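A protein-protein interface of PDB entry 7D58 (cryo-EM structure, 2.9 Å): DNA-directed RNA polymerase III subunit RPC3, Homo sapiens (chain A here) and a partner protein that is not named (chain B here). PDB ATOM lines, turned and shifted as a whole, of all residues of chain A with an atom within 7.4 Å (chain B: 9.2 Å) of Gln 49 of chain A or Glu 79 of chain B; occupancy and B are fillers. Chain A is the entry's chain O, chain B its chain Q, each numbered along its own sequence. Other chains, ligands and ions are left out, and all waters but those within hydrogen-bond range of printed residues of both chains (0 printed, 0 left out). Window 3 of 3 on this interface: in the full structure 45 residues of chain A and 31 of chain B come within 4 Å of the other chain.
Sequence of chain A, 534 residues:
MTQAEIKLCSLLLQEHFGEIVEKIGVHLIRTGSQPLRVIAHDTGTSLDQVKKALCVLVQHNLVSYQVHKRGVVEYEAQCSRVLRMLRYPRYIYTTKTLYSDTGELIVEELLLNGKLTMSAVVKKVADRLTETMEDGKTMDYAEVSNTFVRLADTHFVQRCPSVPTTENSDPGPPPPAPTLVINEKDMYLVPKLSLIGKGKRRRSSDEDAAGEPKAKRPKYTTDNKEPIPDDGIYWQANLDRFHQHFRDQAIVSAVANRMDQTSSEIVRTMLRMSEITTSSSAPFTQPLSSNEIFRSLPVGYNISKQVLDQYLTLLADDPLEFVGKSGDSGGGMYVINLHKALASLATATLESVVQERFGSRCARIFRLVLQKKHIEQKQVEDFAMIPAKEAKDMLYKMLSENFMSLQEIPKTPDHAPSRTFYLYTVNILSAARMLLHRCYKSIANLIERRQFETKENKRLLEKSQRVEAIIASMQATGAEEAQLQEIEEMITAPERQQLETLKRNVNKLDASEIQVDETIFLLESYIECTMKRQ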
ATOM      1  N   ILE A  20      17.451  -7.880  -3.626  1.00  0.00           N
ATOM      2  CA  ILE A  20      16.728  -9.018  -3.064  1.00  0.00           C
ATOM      3  C   ILE A  20      15.723  -8.548  -2.020  1.00  0.00           C
ATOM      4  O   ILE A  20      14.577  -9.011  -1.980  1.00  0.00           O
ATOM      5  CB  ILE A  20      17.715 -10.044  -2.477  1.00  0.00           C
ATOM      6  CG1 ILE A  20      18.534 -10.694  -3.594  1.00  0.00           C
ATOM      7  CG2 ILE A  20      16.974 -11.104  -1.673  1.00  0.00           C
ATOM      8  CD1 ILE A  20      19.406 -11.839  -3.124  1.00  0.00           C
ATOM      9  N   VAL A  21      16.135  -7.610  -1.165  1.00  0.00           N
ATOM     10  CA  VAL A  21      15.239  -7.135  -0.117  1.00  0.00           C
ATOM     11  C   VAL A  21      14.146  -6.242  -0.695  1.00  0.00           C
ATOM     12  O   VAL A  21      12.994  -6.295  -0.245  1.00  0.00           O
ATOM     13  CB  VAL A  21      16.039  -6.425   0.992  1.00  0.00           C
ATOM     14  CG1 VAL A  21      16.892  -5.313   0.413  1.00  0.00           C
ATOM     15  CG2 VAL A  21      15.109  -5.886   2.071  1.00  0.00           C
ATOM     16  N   ILE A  24      11.206  -8.381  -2.135  1.00  0.00           N
ATOM     17  CA  ILE A  24      10.259  -8.841  -1.126  1.00  0.00           C
ATOM     18  C   ILE A  24       9.485  -7.670  -0.534  1.00  0.00           C
ATOM     19  O   ILE A  24       8.319  -7.821  -0.149  1.00  0.00           O
ATOM     20  CB  ILE A  24      10.990  -9.643  -0.034  1.00  0.00           C
ATOM     21  CG1 ILE A  24      12.020 -10.586  -0.661  1.00  0.00           C
ATOM     22  CG2 ILE A  24       9.996 -10.427   0.811  1.00  0.00           C
ATOM     23  CD1 ILE A  24      11.411 -11.680  -1.510  1.00  0.00           C
ATOM     24  N   GLY A  44       9.449 -16.559  -5.371  1.00  0.00           N
ATOM     25  CA  GLY A  44      10.480 -17.283  -6.084  1.00  0.00           C
ATOM     26  C   GLY A  44      11.859 -17.243  -5.462  1.00  0.00           C
ATOM     27  O   GLY A  44      12.803 -17.767  -6.063  1.00  0.00           O
ATOM     28  N   THR A  45      12.006 -16.638  -4.288  1.00  0.00           N
ATOM     29  CA  THR A  45      13.298 -16.489  -3.636  1.00  0.00           C
ATOM     30  C   THR A  45      13.441 -17.519  -2.516  1.00  0.00           C
ATOM     31  O   THR A  45      12.463 -17.927  -1.885  1.00  0.00           O
ATOM     32  CB  THR A  45      13.453 -15.069  -3.080  1.00  0.00           C
ATOM     33  OG1 THR A  45      13.211 -14.120  -4.124  1.00  0.00           O
ATOM     34  CG2 THR A  45      14.863 -14.841  -2.543  1.00  0.00           C
ATOM     35  N   SER A  46      14.681 -17.944  -2.283  1.00  0.00           N
ATOM     36  CA  SER A  46      14.957 -18.957  -1.272  1.00  0.00           C
ATOM     37  C   SER A  46      14.623 -18.445   0.128  1.00  0.00           C
ATOM     38  O   SER A  46      14.410 -17.250   0.345  1.00  0.00           O
ATOM     39  CB  SER A  46      16.421 -19.391  -1.343  1.00  0.00           C
ATOM     40  OG  SER A  46      16.720 -20.341  -0.336  1.00  0.00           O
ATOM     41  N   LEU A  47      14.585 -19.377   1.085  1.00  0.00           N
ATOM     42  CA  LEU A  47      14.094 -19.062   2.425  1.00  0.00           C
ATOM     43  C   LEU A  47      15.069 -18.165   3.185  1.00  0.00           C
ATOM     44  O   LEU A  47      14.656 -17.242   3.896  1.00  0.00           O
ATOM     45  CB  LEU A  47      13.838 -20.359   3.197  1.00  0.00           C
ATOM     46  CG  LEU A  47      12.510 -21.076   2.951  1.00  0.00           C
ATOM     47  CD1 LEU A  47      12.479 -22.402   3.692  1.00  0.00           C
ATOM     48  CD2 LEU A  47      11.340 -20.202   3.371  1.00  0.00           C
ATOM     49  N   ASP A  48      16.371 -18.426   3.043  1.00  0.00           N
ATOM     50  CA  ASP A  48      17.369 -17.675   3.803  1.00  0.00           C
ATOM     51  C   ASP A  48      17.384 -16.205   3.397  1.00  0.00           C
ATOM     52  O   ASP A  48      17.409 -15.310   4.251  1.00  0.00           O
ATOM     53  CB  ASP A  48      18.750 -18.305   3.618  1.00  0.00           C
ATOM     54  CG  ASP A  48      19.007 -18.750   2.191  1.00  0.00           C
ATOM     55  OD1 ASP A  48      20.124 -19.236   1.916  1.00  0.00           O
ATOM     56  OD2 ASP A  48      18.095 -18.623   1.346  1.00  0.00           O
ATOM     57  N   GLN A  49      17.375 -15.938   2.090  1.00  0.00           N
ATOM     58  CA  GLN A  49      17.376 -14.558   1.620  1.00  0.00           C
ATOM     59  C   GLN A  49      16.077 -13.847   1.982  1.00  0.00           C
ATOM     60  O   GLN A  49      16.079 -12.644   2.268  1.00  0.00           O
ATOM     61  CB  GLN A  49      17.610 -14.523   0.112  1.00  0.00           C
ATOM     62  CG  GLN A  49      18.995 -14.990  -0.301  1.00  0.00           C
ATOM     63  CD  GLN A  49      19.077 -15.325  -1.777  1.00  0.00           C
ATOM     64  OE1 GLN A  49      18.084 -15.715  -2.392  1.00  0.00           O
ATOM     65  NE2 GLN A  49      20.264 -15.179  -2.353  1.00  0.00           N
ATOM     66  N   VAL A  50      14.956 -14.573   1.979  1.00  0.00           N
ATOM     67  CA  VAL A  50      13.691 -13.971   2.384  1.00  0.00           C
ATOM     68  C   VAL A  50      13.726 -13.596   3.859  1.00  0.00           C
ATOM     69  O   VAL A  50      13.260 -12.516   4.242  1.00  0.00           O
ATOM     70  CB  VAL A  50      12.518 -14.916   2.063  1.00  0.00           C
ATOM     71  CG1 VAL A  50      11.271 -14.505   2.832  1.00  0.00           C
ATOM     72  CG2 VAL A  50      12.238 -14.920   0.569  1.00  0.00           C
ATOM     73  N   LYS A  51      14.283 -14.463   4.710  1.00  0.00           N
ATOM     74  CA  LYS A  51      14.418 -14.117   6.121  1.00  0.00           C
ATOM     75  C   LYS A  51      15.356 -12.933   6.320  1.00  0.00           C
ATOM     76  O   LYS A  51      15.096 -12.076   7.175  1.00  0.00           O
ATOM     77  CB  LYS A  51      14.910 -15.327   6.913  1.00  0.00           C
ATOM     78  CG  LYS A  51      13.889 -16.447   7.021  1.00  0.00           C
ATOM     79  CD  LYS A  51      14.438 -17.610   7.823  1.00  0.00           C
ATOM     80  CE  LYS A  51      15.670 -18.201   7.157  1.00  0.00           C
ATOM     81  NZ  LYS A  51      16.194 -19.374   7.907  1.00  0.00           N
ATOM     82  N   LYS A  52      16.440 -12.865   5.545  1.00  0.00           N
ATOM     83  CA  LYS A  52      17.328 -11.706   5.609  1.00  0.00           C
ATOM     84  C   LYS A  52      16.598 -10.420   5.234  1.00  0.00           C
ATOM     85  O   LYS A  52      16.719  -9.407   5.933  1.00  0.00           O
ATOM     86  CB  LYS A  52      18.539 -11.917   4.699  1.00  0.00           C
ATOM     87  CG  LYS A  52      19.499 -12.989   5.186  1.00  0.00           C
ATOM     88  CD  LYS A  52      20.681 -13.142   4.244  1.00  0.00           C
ATOM     89  CE  LYS A  52      21.568 -14.301   4.668  1.00  0.00           C
ATOM     90  NZ  LYS A  52      22.715 -14.488   3.739  1.00  0.00           N
ATOM     91  N   ALA A  53      15.840 -10.443   4.136  1.00  0.00           N
ATOM     92  CA  ALA A  53      15.066  -9.272   3.740  1.00  0.00           C
ATOM     93  C   ALA A  53      14.055  -8.888   4.812  1.00  0.00           C
ATOM     94  O   ALA A  53      13.869  -7.700   5.105  1.00  0.00           O
ATOM     95  CB  ALA A  53      14.361  -9.539   2.410  1.00  0.00           C
ATOM     96  N   LEU A  54      13.403  -9.882   5.418  1.00  0.00           N
ATOM     97  CA  LEU A  54      12.391  -9.600   6.429  1.00  0.00           C
ATOM     98  C   LEU A  54      13.012  -8.966   7.666  1.00  0.00           C
ATOM     99  O   LEU A  54      12.464  -8.012   8.228  1.00  0.00           O
ATOM    100  CB  LEU A  54      11.643 -10.882   6.792  1.00  0.00           C
ATOM    101  CG  LEU A  54      10.590 -11.349   5.785  1.00  0.00           C
ATOM    102  CD1 LEU A  54       9.921 -12.626   6.265  1.00  0.00           C
ATOM    103  CD2 LEU A  54       9.558 -10.258   5.531  1.00  0.00           C
ATOM    104  N   CYS A  55      14.165  -9.477   8.107  1.00  0.00           N
ATOM    105  CA  CYS A  55      14.796  -8.919   9.299  1.00  0.00           C
ATOM    106  C   CYS A  55      15.386  -7.543   9.009  1.00  0.00           C
ATOM    107  O   CYS A  55      15.442  -6.680   9.891  1.00  0.00           O
ATOM    108  CB  CYS A  55      15.865  -9.868   9.842  1.00  0.00           C
ATOM    109  SG  CYS A  55      17.345 -10.035   8.828  1.00  0.00           S
ATOM    110  N   ILE B  75      22.268  -5.249   1.090  1.00  0.00           N
ATOM    111  CA  ILE B  75      22.734  -6.544   0.610  1.00  0.00           C
ATOM    112  C   ILE B  75      23.329  -6.384  -0.782  1.00  0.00           C
ATOM    113  O   ILE B  75      22.601  -6.328  -1.779  1.00  0.00           O
ATOM    114  CB  ILE B  75      21.595  -7.579   0.612  1.00  0.00           C
ATOM    115  CG1 ILE B  75      21.053  -7.764   2.031  1.00  0.00           C
ATOM    116  CG2 ILE B  75      22.080  -8.909   0.052  1.00  0.00           C
ATOM    117  CD1 ILE B  75      19.787  -8.585   2.098  1.00  0.00           C
ATOM    118  N   GLU B  76      24.656  -6.307  -0.859  1.00  0.00           N
ATOM    119  CA  GLU B  76      25.363  -6.255  -2.131  1.00  0.00           C
ATOM    120  C   GLU B  76      25.851  -7.627  -2.567  1.00  0.00           C
ATOM    121  O   GLU B  76      26.696  -7.720  -3.463  1.00  0.00           O
ATOM    122  CB  GLU B  76      26.541  -5.280  -2.047  1.00  0.00           C
ATOM    123  CG  GLU B  76      27.654  -5.718  -1.106  1.00  0.00           C
ATOM    124  CD  GLU B  76      27.614  -4.995   0.227  1.00  0.00           C
ATOM    125  OE1 GLU B  76      26.644  -4.250   0.472  1.00  0.00           O
ATOM    126  OE2 GLU B  76      28.554  -5.172   1.030  1.00  0.00           O
ATOM    127  N   THR B  77      25.334  -8.691  -1.961  1.00  0.00           N
ATOM    128  CA  THR B  77      25.754 -10.061  -2.251  1.00  0.00           C
ATOM    129  C   THR B  77      24.539 -10.905  -2.628  1.00  0.00           C
ATOM    130  O   THR B  77      24.035 -11.701  -1.826  1.00  0.00           O
ATOM    131  CB  THR B  77      26.525 -10.651  -1.066  1.00  0.00           C
ATOM    132  OG1 THR B  77      26.874 -12.016  -1.334  1.00  0.00           O
ATOM    133  CG2 THR B  77      25.748 -10.521   0.257  1.00  0.00           C
ATOM    134  N   PRO B  78      24.038 -10.753  -3.860  1.00  0.00           N
ATOM    135  CA  PRO B  78      22.911 -11.605  -4.274  1.00  0.00           C
ATOM    136  C   PRO B  78      23.270 -13.079  -4.278  1.00  0.00           C
ATOM    137  O   PRO B  78      22.688 -13.844  -3.501  1.00  0.00           O
ATOM    138  CB  PRO B  78      22.579 -11.086  -5.682  1.00  0.00           C
ATOM    139  CG  PRO B  78      23.833 -10.430  -6.158  1.00  0.00           C
ATOM    140  CD  PRO B  78      24.516  -9.877  -4.943  1.00  0.00           C
ATOM    141  N   GLU B  79      24.236 -13.472  -5.112  1.00  0.00           N
ATOM    142  CA  GLU B  79      25.007 -14.711  -5.077  1.00  0.00           C
ATOM    143  C   GLU B  79      26.115 -14.572  -6.109  1.00  0.00           C
ATOM    144  O   GLU B  79      25.904 -13.985  -7.173  1.00  0.00           O
ATOM    145  CB  GLU B  79      24.195 -15.983  -5.380  1.00  0.00           C
ATOM    146  CG  GLU B  79      23.336 -16.526  -4.241  1.00  0.00           C
ATOM    147  CD  GLU B  79      24.160 -16.937  -3.034  1.00  0.00           C
ATOM    148  OE1 GLU B  79      25.312 -17.383  -3.220  1.00  0.00           O
ATOM    149  OE2 GLU B  79      23.660 -16.812  -1.896  1.00  0.00           O
ATOM    150  N   GLU B  80      27.287 -15.113  -5.797  1.00  0.00           N
ATOM    151  CA  GLU B  80      28.425 -15.062  -6.711  1.00  0.00           C
ATOM    152  C   GLU B  80      28.810 -16.489  -7.080  1.00  0.00           C
ATOM    153  O   GLU B  80      28.939 -17.351  -6.206  1.00  0.00           O
ATOM    154  CB  GLU B  80      29.605 -14.299  -6.102  1.00  0.00           C
ATOM    155  CG  GLU B  80      30.226 -14.937  -4.863  1.00  0.00           C
ATOM    156  CD  GLU B  80      29.554 -14.497  -3.569  1.00  0.00           C
ATOM    157  OE1 GLU B  80      28.461 -13.898  -3.633  1.00  0.00           O
ATOM    158  OE2 GLU B  80      30.118 -14.759  -2.485  1.00  0.00           O
ATOM    159  N   ARG B  81      28.953 -16.740  -8.377  1.00  0.00           N
ATOM    160  CA  ARG B  81      29.293 -18.053  -8.903  1.00  0.00           C
ATOM    161  C   ARG B  81      30.757 -18.084  -9.324  1.00  0.00           C
ATOM    162  O   ARG B  81      31.274 -17.115  -9.890  1.00  0.00           O
ATOM    163  CB  ARG B  81      28.394 -18.409 -10.091  1.00  0.00           C
ATOM    164  CG  ARG B  81      28.598 -19.809 -10.662  1.00  0.00           C
ATOM    165  CD  ARG B  81      28.348 -20.895  -9.621  1.00  0.00           C
ATOM    166  NE  ARG B  81      29.583 -21.551  -9.194  1.00  0.00           N
ATOM    167  CZ  ARG B  81      29.636 -22.576  -8.349  1.00  0.00           C
ATOM    168  NH1 ARG B  81      28.521 -23.075  -7.829  1.00  0.00           N
ATOM    169  NH2 ARG B  81      30.808 -23.103  -8.020  1.00  0.00           N
ATOM    170  N   GLN B  82      31.427 -19.202  -9.032  1.00  0.00           N
ATOM    171  CA  GLN B  82      32.831 -19.387  -9.399  1.00  0.00           C
ATOM    172  C   GLN B  82      32.971 -20.803  -9.953  1.00  0.00           C
ATOM    173  O   GLN B  82      32.681 -21.777  -9.253  1.00  0.00           O
ATOM    174  CB  GLN B  82      33.752 -19.158  -8.209  1.00  0.00           C
ATOM    175  CG  GLN B  82      35.230 -19.379  -8.510  1.00  0.00           C
ATOM    176  CD  GLN B  82      35.757 -18.457  -9.595  1.00  0.00           C
ATOM    177  OE1 GLN B  82      35.927 -18.865 -10.744  1.00  0.00           O
ATOM    178  NE2 GLN B  82      36.024 -17.208  -9.231  1.00  0.00           N
ATOM    179  N   LYS B  96      32.882 -10.657   6.819  1.00  0.00           N
ATOM    180  CA  LYS B  96      31.450 -10.952   6.877  1.00  0.00           C
ATOM    181  C   LYS B  96      30.956 -10.825   8.317  1.00  0.00           C
ATOM    182  O   LYS B  96      30.831 -11.799   9.061  1.00  0.00           O
ATOM    183  CB  LYS B  96      31.176 -12.341   6.315  1.00  0.00           C
ATOM    184  CG  LYS B  96      29.702 -12.687   6.172  1.00  0.00           C
ATOM    185  CD  LYS B  96      29.089 -11.972   4.982  1.00  0.00           C
ATOM    186  CE  LYS B  96      27.696 -12.495   4.670  1.00  0.00           C
ATOM    187  NZ  LYS B  96      26.702 -12.130   5.712  1.00  0.00           N
ATOM    188  N   MET B 110      10.691 -16.900  13.065  1.00  0.00           N
ATOM    189  CA  MET B 110      11.793 -16.726  12.126  1.00  0.00           C
ATOM    190  C   MET B 110      13.133 -16.903  12.829  1.00  0.00           C
ATOM    191  O   MET B 110      13.547 -16.047  13.617  1.00  0.00           O
ATOM    192  CB  MET B 110      11.709 -15.352  11.455  1.00  0.00           C
ATOM    193  CG  MET B 110      12.712 -15.136  10.328  1.00  0.00           C
ATOM    194  SD  MET B 110      14.290 -14.460  10.880  1.00  0.00           S
ATOM    195  CE  MET B 110      13.822 -12.766  11.224  1.00  0.00           C
ATOM    196  N   PRO B 112      17.064 -17.858  11.696  1.00  0.00           N
ATOM    197  CA  PRO B 112      17.993 -18.188  10.612  1.00  0.00           C
ATOM    198  C   PRO B 112      18.965 -19.288  11.011  1.00  0.00           C
ATOM    199  O   PRO B 112      19.103 -19.650  12.181  1.00  0.00           O
ATOM    200  CB  PRO B 112      18.730 -16.866  10.367  1.00  0.00           C
ATOM    201  CG  PRO B 112      18.671 -16.163  11.681  1.00  0.00           C
ATOM    202  CD  PRO B 112      17.347 -16.540  12.290  1.00  0.00           C
ATOM    203  N   ARG B 113      19.644 -19.820   9.999  1.00  0.00           N
ATOM    204  CA  ARG B 113      20.612 -20.893  10.200  1.00  0.00           C
ATOM    205  C   ARG B 113      21.869 -20.377  10.891  1.00  0.00           C
ATOM    206  O   ARG B 113      22.618 -19.580  10.325  1.00  0.00           O
ATOM    207  CB  ARG B 113      20.973 -21.543   8.864  1.00  0.00           C
ATOM    208  CG  ARG B 113      21.985 -22.675   8.969  1.00  0.00           C
ATOM    209  CD  ARG B 113      21.357 -23.936   9.548  1.00  0.00           C
ATOM    210  NE  ARG B 113      21.482 -23.997  11.001  1.00  0.00           N
ATOM    211  CZ  ARG B 113      20.872 -24.897  11.766  1.00  0.00           C
ATOM    212  NH1 ARG B 113      20.089 -25.816  11.217  1.00  0.00           N
ATOM    213  NH2 ARG B 113      21.044 -24.878  13.081  1.00  0.00           N
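The side-chain amide nitrogen (NE2) of Gln 49 of chain A is in hydrogen-bond range of the backbone carbonyl oxygen (O) of Pro 78 of chain B (3.0 Å).
O of Lys 52 of chain A is in hydrogen-bond range of SG of Cys 55 of chain A (3.0 Å). SG of Cys 55 of chain A lies within hydrogen-bond range of O of Lys 51 of chain A (3.5 Å).
Among the printed residues, pairs that only touch across the chains: Ile 20 of chain A with Pro 78 of chain B, Gln 49 of chain A with Glu 79 of chain B, Lys 51 of chain A with Met 110 of chain B, Lys 51 of chain A with Pro 112 of chain B and Cys 55 of chain A with Met 110 of chain B.
Printed residues of chain B within 4 Å of Ile 20 of chain A: Pro 78. Gly 44 of chain A touches none of the printed residues of chain B. No residue of chain B comes within 4 Å of Asp 48 of chain A. Of the printed residues of chain B, Gln 49 of chain A touches Pro 78 (3.0 Å) and Glu 79 (3.8 Å). No residue of chain B comes within 4 Å of Val 50 of chain A. Of the printed residues of chain B, Lys 51 of chain A touches Met 110 and Pro 112. Lys 52 of chain A touches none of the printed residues of chain B. Printed residues of chain B within 4 Å of Cys 55 of chain A: Met 110. Glu 79 of chain B touches just one residue of chain A: Gln 49. Of the printed residues of chain A, Met 110 of chain B touches Lys 51 (3.7 Å) and Cys 55 (3.8 Å). Of the printed residues of chain A, Pro 112 of chain B touches Lys 51 (3.5 Å). The nearest printed residue of chain B that does not touch Lys 51 of chain A is Arg 113 of chain B (4.1 Å).
Of the 12 printed residues of chain B, 4 touch a printed residue of chain A. Printed residues of chain B that touch a printed residue of chain A: Pro 78, Glu 79, Met 110 and Pro 112. Hydrophobic or aromatic side chains of chain B that line the printed part of chain A: Met 110. Among the printed residues, 6 pairs touch across the chains.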
